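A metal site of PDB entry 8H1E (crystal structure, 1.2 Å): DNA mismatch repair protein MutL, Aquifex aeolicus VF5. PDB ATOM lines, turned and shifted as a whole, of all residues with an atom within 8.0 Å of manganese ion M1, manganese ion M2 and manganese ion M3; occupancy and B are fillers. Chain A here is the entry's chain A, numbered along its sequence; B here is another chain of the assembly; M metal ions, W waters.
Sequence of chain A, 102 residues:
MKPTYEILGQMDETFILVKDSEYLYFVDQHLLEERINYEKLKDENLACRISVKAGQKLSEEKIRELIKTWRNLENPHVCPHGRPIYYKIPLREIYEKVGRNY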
ATOM      1  N   ASP A  28      28.887 -11.392  19.706  1.00  0.00           N
ATOM      2  CA  ASP A  28      28.321 -12.670  20.133  1.00  0.00           C
ATOM      3  C   ASP A  28      28.327 -13.634  18.952  1.00  0.00           C
ATOM      4  O   ASP A  28      27.639 -13.393  17.952  1.00  0.00           O
ATOM      5  CB  ASP A  28      26.877 -12.436  20.621  1.00  0.00           C
ATOM      6  CG  ASP A  28      26.249 -13.654  21.252  1.00  0.00           C
ATOM      7  OD1 ASP A  28      26.196 -14.713  20.600  1.00  0.00           O
ATOM      8  OD2 ASP A  28      25.759 -13.531  22.388  1.00  0.00           O
ATOM      9  N   HIS A  30      27.017 -16.594  18.470  1.00  0.00           N
ATOM     10  CA  HIS A  30      25.726 -17.183  18.118  1.00  0.00           C
ATOM     11  C   HIS A  30      24.852 -16.167  17.407  1.00  0.00           C
ATOM     12  O   HIS A  30      24.268 -16.454  16.346  1.00  0.00           O
ATOM     13  CB  HIS A  30      24.994 -17.706  19.337  1.00  0.00           C
ATOM     14  CG  HIS A  30      23.576 -18.076  19.036  1.00  0.00           C
ATOM     15  ND1 HIS A  30      23.252 -19.215  18.333  1.00  0.00           N
ATOM     16  CD2 HIS A  30      22.408 -17.431  19.257  1.00  0.00           C
ATOM     17  CE1 HIS A  30      21.935 -19.279  18.182  1.00  0.00           C
ATOM     18  NE2 HIS A  30      21.405 -18.205  18.727  1.00  0.00           N
ATOM     19  N   LEU A  31      24.728 -14.962  17.982  1.00  0.00           N
ATOM     20  CA  LEU A  31      23.857 -13.957  17.384  1.00  0.00           C
ATOM     21  C   LEU A  31      24.355 -13.540  16.001  1.00  0.00           C
ATOM     22  O   LEU A  31      23.541 -13.301  15.093  1.00  0.00           O
ATOM     23  CB  LEU A  31      23.767 -12.728  18.286  1.00  0.00           C
ATOM     24  CG  LEU A  31      23.075 -12.861  19.649  1.00  0.00           C
ATOM     25  CD1 LEU A  31      23.060 -11.534  20.378  1.00  0.00           C
ATOM     26  CD2 LEU A  31      21.672 -13.410  19.550  1.00  0.00           C
ATOM     27  N   LEU A  32      25.676 -13.474  15.803  1.00  0.00           N
ATOM     28  CA  LEU A  32      26.204 -13.137  14.480  1.00  0.00           C
ATOM     29  C   LEU A  32      25.868 -14.217  13.466  1.00  0.00           C
ATOM     30  O   LEU A  32      25.335 -13.914  12.386  1.00  0.00           O
ATOM     31  CB  LEU A  32      27.709 -12.922  14.559  1.00  0.00           C
ATOM     32  CG  LEU A  32      28.442 -12.772  13.233  1.00  0.00           C
ATOM     33  CD1 LEU A  32      27.818 -11.661  12.376  1.00  0.00           C
ATOM     34  CD2 LEU A  32      29.948 -12.532  13.428  1.00  0.00           C
ATOM     35  N   GLU A  34      23.549 -16.417  13.620  1.00  0.00           N
ATOM     36  CA  GLU A  34      22.103 -16.435  13.442  1.00  0.00           C
ATOM     37  C   GLU A  34      21.663 -15.343  12.477  1.00  0.00           C
ATOM     38  O   GLU A  34      20.791 -15.565  11.639  1.00  0.00           O
ATOM     39  CB  GLU A  34      21.400 -16.256  14.787  1.00  0.00           C
ATOM     40  CG  GLU A  34      19.879 -16.346  14.756  1.00  0.00           C
ATOM     41  CD  GLU A  34      19.253 -15.980  16.099  1.00  0.00           C
ATOM     42  OE1 GLU A  34      19.292 -14.790  16.492  1.00  0.00           O
ATOM     43  OE2 GLU A  34      18.775 -16.904  16.782  1.00  0.00           O
ATOM     44  N   ARG A  35      22.274 -14.167  12.590  1.00  0.00           N
ATOM     45  CA  ARG A  35      21.967 -13.077  11.658  1.00  0.00           C
ATOM     46  C   ARG A  35      22.405 -13.420  10.235  1.00  0.00           C
ATOM     47  O   ARG A  35      21.648 -13.205   9.277  1.00  0.00           O
ATOM     48  CB  ARG A  35      22.584 -11.772  12.145  1.00  0.00           C
ATOM     49  CG  ARG A  35      22.191 -10.553  11.318  1.00  0.00           C
ATOM     50  CD  ARG A  35      20.819 -10.056  11.756  1.00  0.00           C
ATOM     51  NE  ARG A  35      20.017  -9.572  10.644  1.00  0.00           N
ATOM     52  CZ  ARG A  35      18.799  -9.070  10.783  1.00  0.00           C
ATOM     53  NH1 ARG A  35      18.236  -8.920  11.972  1.00  0.00           N
ATOM     54  NH2 ARG A  35      18.112  -8.715   9.697  1.00  0.00           N
ATOM     55  N   GLU A  44      13.746 -17.386  11.024  1.00  0.00           N
ATOM     56  CA  GLU A  44      14.496 -17.145  12.258  1.00  0.00           C
ATOM     57  C   GLU A  44      14.665 -18.411  13.100  1.00  0.00           C
ATOM     58  O   GLU A  44      15.690 -18.556  13.772  1.00  0.00           O
ATOM     59  CB  GLU A  44      13.892 -15.980  13.062  1.00  0.00           C
ATOM     60  CG  GLU A  44      12.899 -16.401  14.114  1.00  0.00           C
ATOM     61  CD  GLU A  44      12.360 -15.219  14.919  1.00  0.00           C
ATOM     62  OE1 GLU A  44      12.600 -14.061  14.513  1.00  0.00           O
ATOM     63  OE2 GLU A  44      11.682 -15.469  15.936  1.00  0.00           O
ATOM     64  N   ASN A  45      13.703 -19.328  13.050  1.00  0.00           N
ATOM     65  CA  ASN A  45      13.832 -20.564  13.816  1.00  0.00           C
ATOM     66  C   ASN A  45      14.928 -21.440  13.225  1.00  0.00           C
ATOM     67  O   ASN A  45      15.748 -22.016  13.956  1.00  0.00           O
ATOM     68  CB  ASN A  45      12.510 -21.333  13.790  1.00  0.00           C
ATOM     69  CG  ASN A  45      11.495 -20.765  14.742  1.00  0.00           C
ATOM     70  OD1 ASN A  45      11.787 -19.865  15.520  1.00  0.00           O
ATOM     71  ND2 ASN A  45      10.276 -21.309  14.707  1.00  0.00           N
ATOM     72  N   LEU A  46      14.957 -21.544  11.899  1.00  0.00           N
ATOM     73  CA  LEU A  46      15.974 -22.359  11.243  1.00  0.00           C
ATOM     74  C   LEU A  46      17.345 -21.725  11.412  1.00  0.00           C
ATOM     75  O   LEU A  46      18.334 -22.415  11.695  1.00  0.00           O
ATOM     76  CB  LEU A  46      15.640 -22.500   9.755  1.00  0.00           C
ATOM     77  CG  LEU A  46      16.617 -23.352   8.925  1.00  0.00           C
ATOM     78  CD1 LEU A  46      16.670 -24.752   9.482  1.00  0.00           C
ATOM     79  CD2 LEU A  46      16.273 -23.381   7.446  1.00  0.00           C
ATOM     80  N   ALA A  47      17.421 -20.410  11.229  1.00  0.00           N
ATOM     81  CA  ALA A  47      18.697 -19.719  11.403  1.00  0.00           C
ATOM     82  C   ALA A  47      19.251 -19.944  12.806  1.00  0.00           C
ATOM     83  O   ALA A  47      20.449 -20.187  12.974  1.00  0.00           O
ATOM     84  CB  ALA A  47      18.529 -18.226  11.111  1.00  0.00           C
ATOM     85  N   CYS A  48      18.392 -19.895  13.816  1.00  0.00           N
ATOM     86  CA  CYS A  48      18.858 -20.076  15.186  1.00  0.00           C
ATOM     87  C   CYS A  48      19.392 -21.493  15.383  1.00  0.00           C
ATOM     88  O   CYS A  48      20.497 -21.670  15.895  1.00  0.00           O
ATOM     89  CB  CYS A  48      17.722 -19.800  16.164  1.00  0.00           C
ATOM     90  SG  CYS A  48      18.213 -20.111  17.895  1.00  0.00           S
ATOM     91  N   ARG A  49      18.622 -22.515  14.959  1.00  0.00           N
ATOM     92  CA  ARG A  49      18.933 -23.890  15.342  1.00  0.00           C
ATOM     93  C   ARG A  49      20.194 -24.418  14.646  1.00  0.00           C
ATOM     94  O   ARG A  49      20.852 -25.335  15.175  1.00  0.00           O
ATOM     95  CB  ARG A  49      17.751 -24.826  15.075  1.00  0.00           C
ATOM     96  CG  ARG A  49      17.522 -25.182  13.602  1.00  0.00           C
ATOM     97  CD  ARG A  49      16.108 -25.622  13.337  1.00  0.00           C
ATOM     98  NE  ARG A  49      15.739 -26.816  14.080  1.00  0.00           N
ATOM     99  CZ  ARG A  49      14.509 -27.321  14.120  1.00  0.00           C
ATOM    100  NH1 ARG A  49      13.501 -26.734  13.486  1.00  0.00           N
ATOM    101  NH2 ARG A  49      14.290 -28.452  14.792  1.00  0.00           N
ATOM    102  N   SER A  51      22.866 -22.445  13.866  1.00  0.00           N
ATOM    103  CA  SER A  51      24.017 -21.609  14.150  1.00  0.00           C
ATOM    104  C   SER A  51      24.843 -22.144  15.313  1.00  0.00           C
ATOM    105  O   SER A  51      24.374 -22.941  16.130  1.00  0.00           O
ATOM    106  CB  SER A  51      23.551 -20.210  14.508  1.00  0.00           C
ATOM    107  OG  SER A  51      22.955 -19.593  13.402  1.00  0.00           O
ATOM    108  N   VAL A  52      26.104 -21.719  15.332  1.00  0.00           N
ATOM    109  CA  VAL A  52      26.982 -22.046  16.436  1.00  0.00           C
ATOM    110  C   VAL A  52      26.375 -21.536  17.739  1.00  0.00           C
ATOM    111  O   VAL A  52      25.646 -20.541  17.780  1.00  0.00           O
ATOM    112  CB  VAL A  52      28.377 -21.424  16.223  1.00  0.00           C
ATOM    113  CG1 VAL A  52      28.312 -19.907  16.329  1.00  0.00           C
ATOM    114  CG2 VAL A  52      29.359 -21.987  17.214  1.00  0.00           C
ATOM    115  N   LYS A  53      26.664 -22.230  18.823  1.00  0.00           N
ATOM    116  CA  LYS A  53      26.226 -21.817  20.147  1.00  0.00           C
ATOM    117  C   LYS A  53      27.385 -21.246  20.940  1.00  0.00           C
ATOM    118  O   LYS A  53      28.555 -21.491  20.649  1.00  0.00           O
ATOM    119  CB  LYS A  53      25.613 -22.991  20.885  1.00  0.00           C
ATOM    120  CG  LYS A  53      24.368 -23.499  20.187  1.00  0.00           C
ATOM    121  CD  LYS A  53      23.705 -24.626  20.930  1.00  0.00           C
ATOM    122  CE  LYS A  53      22.617 -25.254  20.077  1.00  0.00           C
ATOM    123  NZ  LYS A  53      21.591 -24.282  19.629  1.00  0.00           N
ATOM    124  N   VAL A  78      21.504  -6.016  15.193  1.00  0.00           N
ATOM    125  CA  VAL A  78      20.634  -6.806  16.054  1.00  0.00           C
ATOM    126  C   VAL A  78      20.293  -8.115  15.362  1.00  0.00           C
ATOM    127  O   VAL A  78      20.206  -8.186  14.137  1.00  0.00           O
ATOM    128  CB  VAL A  78      19.349  -6.038  16.412  1.00  0.00           C
ATOM    129  CG1 VAL A  78      19.648  -4.948  17.443  1.00  0.00           C
ATOM    130  CG2 VAL A  78      18.664  -5.489  15.161  1.00  0.00           C
ATOM    131  N   CYS A  79      20.086  -9.156  16.165  1.00  0.00           N
ATOM    132  CA  CYS A  79      19.697 -10.443  15.593  1.00  0.00           C
ATOM    133  C   CYS A  79      18.211 -10.362  15.239  1.00  0.00           C
ATOM    134  O   CYS A  79      17.546  -9.356  15.533  1.00  0.00           O
ATOM    135  CB  CYS A  79      19.901 -11.568  16.621  1.00  0.00           C
ATOM    136  SG  CYS A  79      18.699 -11.648  17.975  1.00  0.00           S
ATOM    137  N   PRO A  80      17.654 -11.392  14.574  1.00  0.00           N
ATOM    138  CA  PRO A  80      16.225 -11.336  14.225  1.00  0.00           C
ATOM    139  C   PRO A  80      15.283 -11.174  15.412  1.00  0.00           C
ATOM    140  O   PRO A  80      14.150 -10.735  15.224  1.00  0.00           O
ATOM    141  CB  PRO A  80      15.950 -12.675  13.512  1.00  0.00           C
ATOM    142  CG  PRO A  80      17.202 -13.425  13.508  1.00  0.00           C
ATOM    143  CD  PRO A  80      18.328 -12.541  13.938  1.00  0.00           C
ATOM    144  N   HIS A  81      15.704 -11.558  16.614  1.00  0.00           N
ATOM    145  CA  HIS A  81      14.916 -11.353  17.822  1.00  0.00           C
ATOM    146  C   HIS A  81      15.143  -9.989  18.457  1.00  0.00           C
ATOM    147  O   HIS A  81      14.517  -9.691  19.473  1.00  0.00           O
ATOM    148  CB  HIS A  81      15.212 -12.445  18.848  1.00  0.00           C
ATOM    149  CG  HIS A  81      15.066 -13.824  18.292  1.00  0.00           C
ATOM    150  ND1 HIS A  81      16.137 -14.559  17.830  1.00  0.00           N
ATOM    151  CD2 HIS A  81      13.968 -14.597  18.106  1.00  0.00           C
ATOM    152  CE1 HIS A  81      15.700 -15.730  17.393  1.00  0.00           C
ATOM    153  NE2 HIS A  81      14.388 -15.779  17.559  1.00  0.00           N
ATOM    154  N   GLY A  82      16.023  -9.166  17.889  1.00  0.00           N
ATOM    155  CA  GLY A  82      16.242  -7.823  18.372  1.00  0.00           C
ATOM    156  C   GLY A  82      17.323  -7.682  19.419  1.00  0.00           C
ATOM    157  O   GLY A  82      17.481  -6.589  19.965  1.00  0.00           O
ATOM    158  N   ARG A  83      18.063  -8.753  19.736  1.00  0.00           N
ATOM    159  CA  ARG A  83      19.149  -8.592  20.705  1.00  0.00           C
ATOM    160  C   ARG A  83      20.363  -7.965  20.012  1.00  0.00           C
ATOM    161  O   ARG A  83      20.695  -8.343  18.891  1.00  0.00           O
ATOM    162  CB  ARG A  83      19.580  -9.953  21.266  1.00  0.00           C
ATOM    163  CG  ARG A  83      18.505 -10.685  22.066  1.00  0.00           C
ATOM    164  CD  ARG A  83      19.104 -11.927  22.717  1.00  0.00           C
ATOM    165  N   PRO A  84      21.041  -7.019  20.654  1.00  0.00           N
ATOM    166  CA  PRO A  84      22.296  -6.496  20.095  1.00  0.00           C
ATOM    167  C   PRO A  84      23.289  -7.619  19.813  1.00  0.00           C
ATOM    168  O   PRO A  84      23.526  -8.484  20.666  1.00  0.00           O
ATOM    169  CB  PRO A  84      22.807  -5.539  21.181  1.00  0.00           C
ATOM    170  CG  PRO A  84      21.559  -5.133  21.926  1.00  0.00           C
ATOM    171  CD  PRO A  84      20.684  -6.353  21.921  1.00  0.00           C
ATOM    172  N   ILE A  85      23.880  -7.586  18.625  1.00  0.00           N
ATOM    173  CA  ILE A  85      24.828  -8.617  18.209  1.00  0.00           C
ATOM    174  C   ILE A  85      26.146  -8.455  18.933  1.00  0.00           C
ATOM    175  O   ILE A  85      26.889  -9.424  19.102  1.00  0.00           O
ATOM    176  CB  ILE A  85      24.980  -8.622  16.675  1.00  0.00           C
ATOM    177  CG1 ILE A  85      23.693  -9.140  16.016  1.00  0.00           C
ATOM    178  CG2 ILE A  85      26.220  -9.413  16.215  1.00  0.00           C
ATOM    179  CD1 ILE A  85      23.722  -9.029  14.520  1.00  0.00           C
ATOM    180  N   VAL B  98      24.153  -8.297  25.141  1.00  0.00           N
ATOM    181  CA  VAL B  98      23.724  -9.250  24.121  1.00  0.00           C
ATOM    182  C   VAL B  98      22.633 -10.172  24.653  1.00  0.00           C
ATOM    183  O   VAL B  98      22.279 -11.170  24.000  1.00  0.00           O
ATOM    184  CB  VAL B  98      24.926 -10.025  23.522  1.00  0.00           C
ATOM    185  CG1 VAL B  98      25.934  -9.075  22.885  1.00  0.00           C
ATOM    186  CG2 VAL B  98      25.616 -10.905  24.583  1.00  0.00           C
ATOM    187  N   ARG B 100      22.573 -12.033  27.555  1.00  0.00           N
ATOM    188  CA  ARG B 100      23.003 -13.261  28.223  1.00  0.00           C
ATOM    189  C   ARG B 100      23.151 -13.030  29.729  1.00  0.00           C
ATOM    190  O   ARG B 100      23.543 -11.942  30.185  1.00  0.00           O
ATOM    191  CB  ARG B 100      24.361 -13.741  27.700  1.00  0.00           C
ATOM    192  CG  ARG B 100      24.347 -14.231  26.273  1.00  0.00           C
ATOM    193  CD  ARG B 100      25.704 -14.781  25.849  1.00  0.00           C
ATOM    194  NE  ARG B 100      25.652 -15.216  24.462  1.00  0.00           N
ATOM    195  CZ  ARG B 100      25.151 -16.384  24.064  1.00  0.00           C
ATOM    196  NH1 ARG B 100      24.770 -17.302  24.938  1.00  0.00           N
ATOM    197  NH2 ARG B 100      25.013 -16.618  22.770  1.00  0.00           N
HETATM  198 MN    MN M   1      19.116 -17.924  18.809  1.00  0.00          MN
HETATM  199 MN    MN M   2      18.297 -14.090  18.184  1.00  0.00          MN
HETATM  200 MN    MN M   3      16.063 -20.024  19.272  1.00  0.00          MN
HETATM  201  O   HOH W   1      19.281 -18.744  20.883  1.00  0.00           O
HETATM  202  O   HOH W   2      17.956 -14.082  20.407  1.00  0.00           O
HETATM  203  O   HOH W   3      16.689 -17.692  19.906  1.00  0.00           O
HETATM  204  O   HOH W   4      14.433 -21.292  18.456  1.00  0.00           O
HETATM  205  O   HOH W   5      19.160 -15.723  19.549  1.00  0.00           O
HETATM  206  O   HOH W   6      14.394 -18.986  17.239  1.00  0.00           O
HETATM  207  O   HOH W   7      16.670 -20.322  21.387  1.00  0.00           O
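The backbone NH (N) of Glu 34 lies within hydrogen-bond range of the side-chain hydroxyl (OG) of Ser 51, at 3.2 Å. The side-chain carboxylate (OE2) of Glu 44 lies within hydrogen-bond range of a ring nitrogen (NE2) of His 81 (3.2 Å). ND1 of His 30 sits at hydrogen-bond distance from O of Val 52 (2.8 Å). N of His 30 sits at hydrogen-bond distance from OD1 of Asp 28 (3.0 Å). The side-chain sulfur (SG) of Cys 79 lies close to the backbone NH (N) of Arg 83 (3.4 Å). The side-chain sulfur (SG) of Cys 79 sits close to the backbone NH (N) of Gly 82 (3.7 Å). The backbone NH of Leu 31 is in hydrogen-bond range of the side-chain carboxylate of Asp 28, at 3.0 Å.
Of the 25 residues printed, 3 come within 4 Å of manganese ion M1.
CD2 of Leu 31 touches manganese ion M2, at 3.7 Å. Four residues have an atom within 4 Å of manganese ion M2: Leu 31, Glu 34, Cys 79 and His 81. The nearest printed residue that does not touch manganese ion M2 is Pro 80 (4.5 Å).
Of the 25 residues printed, 1 comes within 4 Å of manganese ion M3.
Water W1 binds manganese ion M1. Manganese ion M1 is bound by OE2 of Glu 34 (2.3 Å). NE2 of His 30 is bound to manganese ion M1 (2.3 Å). Water W5 binds manganese ion M1 (2.3 Å). SG of Cys 48 is bound to manganese ion M1 (2.5 Å). Water W3 binds manganese ion M1 (2.7 Å). Manganese ion M1 has six donor atoms within binding distance.
Manganese ion M2 is bound by OE1 of Glu 34 (2.1 Å), ND1 of His 81 (2.2 Å), water W2 (2.2 Å), water W5 (2.3 Å) and SG of Cys 79 (2.5 Å).
Water W4 binds manganese ion M3 (2.2 Å). Manganese ion M3 is bound by water W7 (2.2 Å). Manganese ion M3 is bound by water W3 (2.5 Å). SG of Cys 48 binds manganese ion M3 (2.6 Å). Slightly farther from manganese ion M3 lies water W6 (2.8 Å).
Water W6 bridges a ring nitrogen (NE2) of His 81 (3.2 Å) and the side-chain amide oxygen of Asn 45 (3.2 Å).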
